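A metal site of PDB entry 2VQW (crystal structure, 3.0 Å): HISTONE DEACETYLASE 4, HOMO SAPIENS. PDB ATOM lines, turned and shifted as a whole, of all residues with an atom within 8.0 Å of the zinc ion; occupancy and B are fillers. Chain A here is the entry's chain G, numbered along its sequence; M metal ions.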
ATOM      1  N   GLN A  22       8.024  31.032   9.176  1.00  0.00           N
ATOM      2  CA  GLN A  22       7.739  30.527  10.508  1.00  0.00           C
ATOM      3  C   GLN A  22       8.858  29.602  10.945  1.00  0.00           C
ATOM      4  O   GLN A  22       9.565  29.044  10.107  1.00  0.00           O
ATOM      5  CB  GLN A  22       6.410  29.779  10.531  1.00  0.00           C
ATOM      6  CG  GLN A  22       5.174  30.659  10.558  1.00  0.00           C
ATOM      7  CD  GLN A  22       3.881  29.860  10.477  1.00  0.00           C
ATOM      8  OE1 GLN A  22       3.684  28.908  11.238  1.00  0.00           O
ATOM      9  NE2 GLN A  22       2.994  30.251   9.566  1.00  0.00           N
ATOM     10  N   CYS A  23       9.027  29.458  12.259  1.00  0.00           N
ATOM     11  CA  CYS A  23      10.062  28.565  12.793  1.00  0.00           C
ATOM     12  C   CYS A  23       9.781  27.122  12.420  1.00  0.00           C
ATOM     13  O   CYS A  23       8.617  26.701  12.360  1.00  0.00           O
ATOM     14  CB  CYS A  23      10.162  28.682  14.318  1.00  0.00           C
ATOM     15  SG  CYS A  23      11.538  27.742  14.992  1.00  0.00           S
ATOM     16  N   THR A  24      10.853  26.370  12.185  1.00  0.00           N
ATOM     17  CA  THR A  24      10.758  24.979  11.734  1.00  0.00           C
ATOM     18  C   THR A  24      10.036  24.062  12.735  1.00  0.00           C
ATOM     19  O   THR A  24       9.595  22.979  12.373  1.00  0.00           O
ATOM     20  CB  THR A  24      12.142  24.389  11.379  1.00  0.00           C
ATOM     21  OG1 THR A  24      13.023  24.541  12.501  1.00  0.00           O
ATOM     22  CG2 THR A  24      12.730  25.094  10.157  1.00  0.00           C
ATOM     23  N   CYS A  25       9.922  24.517  13.983  1.00  0.00           N
ATOM     24  CA  CYS A  25       9.055  23.855  14.958  1.00  0.00           C
ATOM     25  C   CYS A  25       7.634  24.393  14.796  1.00  0.00           C
ATOM     26  O   CYS A  25       6.748  24.097  15.598  1.00  0.00           O
ATOM     27  CB  CYS A  25       9.567  24.056  16.387  1.00  0.00           C
ATOM     28  SG  CYS A  25       9.397  25.737  17.064  1.00  0.00           S
ATOM     29  N   SER A  29       4.558  30.607  18.897  1.00  0.00           N
ATOM     30  CA  SER A  29       4.890  29.612  19.917  1.00  0.00           C
ATOM     31  C   SER A  29       5.629  30.266  21.091  1.00  0.00           C
ATOM     32  O   SER A  29       5.010  30.811  22.003  1.00  0.00           O
ATOM     33  CB  SER A  29       5.727  28.478  19.295  1.00  0.00           C
ATOM     34  OG  SER A  29       5.140  27.988  18.096  1.00  0.00           O
ATOM     35  N   SER A  30       6.962  30.201  21.078  1.00  0.00           N
ATOM     36  CA  SER A  30       7.806  30.971  21.985  1.00  0.00           C
ATOM     37  C   SER A  30       8.470  32.121  21.218  1.00  0.00           C
ATOM     38  O   SER A  30       9.532  32.620  21.590  1.00  0.00           O
ATOM     39  CB  SER A  30       8.873  30.073  22.627  1.00  0.00           C
ATOM     40  OG  SER A  30       9.721  29.522  21.636  1.00  0.00           O
ATOM     41  N   HIS A  31       7.806  32.526  20.128  1.00  0.00           N
ATOM     42  CA  HIS A  31       8.293  33.556  19.223  1.00  0.00           C
ATOM     43  C   HIS A  31       7.270  34.678  19.105  1.00  0.00           C
ATOM     44  O   HIS A  31       6.206  34.470  18.519  1.00  0.00           O
ATOM     45  CB  HIS A  31       8.557  32.965  17.839  1.00  0.00           C
ATOM     46  CG  HIS A  31       9.430  31.755  17.861  1.00  0.00           C
ATOM     47  ND1 HIS A  31      10.807  31.831  17.871  1.00  0.00           N
ATOM     48  CD2 HIS A  31       9.133  30.430  17.864  1.00  0.00           C
ATOM     49  CE1 HIS A  31      11.313  30.607  17.892  1.00  0.00           C
ATOM     50  NE2 HIS A  31      10.316  29.738  17.892  1.00  0.00           N
ATOM     51  N   LEU A 105      18.225  26.747  18.060  1.00  0.00           N
ATOM     52  CA  LEU A 105      17.468  27.476  19.074  1.00  0.00           C
ATOM     53  C   LEU A 105      17.140  26.612  20.300  1.00  0.00           C
ATOM     54  O   LEU A 105      17.288  25.394  20.249  1.00  0.00           O
ATOM     55  CB  LEU A 105      16.180  28.055  18.455  1.00  0.00           C
ATOM     56  CG  LEU A 105      16.197  29.518  17.955  1.00  0.00           C
ATOM     57  CD1 LEU A 105      17.345  29.794  17.001  1.00  0.00           C
ATOM     58  CD2 LEU A 105      14.870  29.883  17.305  1.00  0.00           C
ATOM     59  N   PRO A 106      16.707  27.249  21.405  1.00  0.00           N
ATOM     60  CA  PRO A 106      16.282  26.477  22.578  1.00  0.00           C
ATOM     61  C   PRO A 106      14.915  25.805  22.364  1.00  0.00           C
ATOM     62  O   PRO A 106      14.443  25.084  23.245  1.00  0.00           O
ATOM     63  CB  PRO A 106      16.188  27.527  23.679  1.00  0.00           C
ATOM     64  CG  PRO A 106      15.869  28.795  22.961  1.00  0.00           C
ATOM     65  CD  PRO A 106      16.587  28.701  21.652  1.00  0.00           C
ATOM     66  N   CYS A 107      14.303  26.040  21.204  1.00  0.00           N
ATOM     67  CA  CYS A 107      13.023  25.431  20.861  1.00  0.00           C
ATOM     68  C   CYS A 107      13.184  24.295  19.842  1.00  0.00           C
ATOM     69  O   CYS A 107      12.215  23.624  19.485  1.00  0.00           O
ATOM     70  CB  CYS A 107      12.054  26.502  20.334  1.00  0.00           C
ATOM     71  SG  CYS A 107      12.478  27.177  18.699  1.00  0.00           S
ATOM     72  N   GLY A 108      14.412  24.105  19.371  1.00  0.00           N
ATOM     73  CA  GLY A 108      14.708  23.057  18.386  1.00  0.00           C
ATOM     74  C   GLY A 108      14.872  23.570  16.966  1.00  0.00           C
ATOM     75  O   GLY A 108      15.447  22.887  16.125  1.00  0.00           O
ATOM     76  N   GLY A 109      14.364  24.771  16.699  1.00  0.00           N
ATOM     77  CA  GLY A 109      14.407  25.346  15.359  1.00  0.00           C
ATOM     78  C   GLY A 109      15.744  25.937  14.943  1.00  0.00           C
ATOM     79  O   GLY A 109      16.680  26.023  15.735  1.00  0.00           O
ATOM     80  N   VAL A 110      15.821  26.354  13.674  1.00  0.00           N
ATOM     81  CA  VAL A 110      17.004  26.995  13.133  1.00  0.00           C
ATOM     82  C   VAL A 110      16.874  28.507  13.270  1.00  0.00           C
ATOM     83  O   VAL A 110      15.796  29.055  13.072  1.00  0.00           O
ATOM     84  CB  VAL A 110      17.221  26.629  11.653  1.00  0.00           C
ATOM     85  CG1 VAL A 110      18.533  27.217  11.126  1.00  0.00           C
ATOM     86  CG2 VAL A 110      17.213  25.116  11.449  1.00  0.00           C
ATOM     87  N   ILE A 117      14.513  33.790  14.152  1.00  0.00           N
ATOM     88  CA  ILE A 117      14.427  32.495  13.471  1.00  0.00           C
ATOM     89  C   ILE A 117      15.016  32.534  12.073  1.00  0.00           C
ATOM     90  O   ILE A 117      15.404  33.593  11.581  1.00  0.00           O
ATOM     91  CB  ILE A 117      12.971  32.009  13.349  1.00  0.00           C
ATOM     92  CG1 ILE A 117      12.166  32.952  12.456  1.00  0.00           C
ATOM     93  CG2 ILE A 117      12.335  31.849  14.729  1.00  0.00           C
ATOM     94  CD1 ILE A 117      11.074  32.279  11.662  1.00  0.00           C
HETATM   95 ZN    ZN M   1      10.776  27.793  17.210  1.00  0.00          ZN
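SG of Cys 107 lies close to N of Gly 109, at 3.7 Å.
Within 4 Å of the zinc ion: Cys 23, Cys 25, His 31 and Cys 107.
NE2 of His 31 is bound to the zinc ion (2.1 Å).
The zinc ion is bound by SG of Cys 107 (2.3 Å).
SG of Cys 23 binds the zinc ion, 2.3 Å away.
SG of Cys 25 binds the zinc ion.
The zinc ion has four donor atoms within binding distance.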
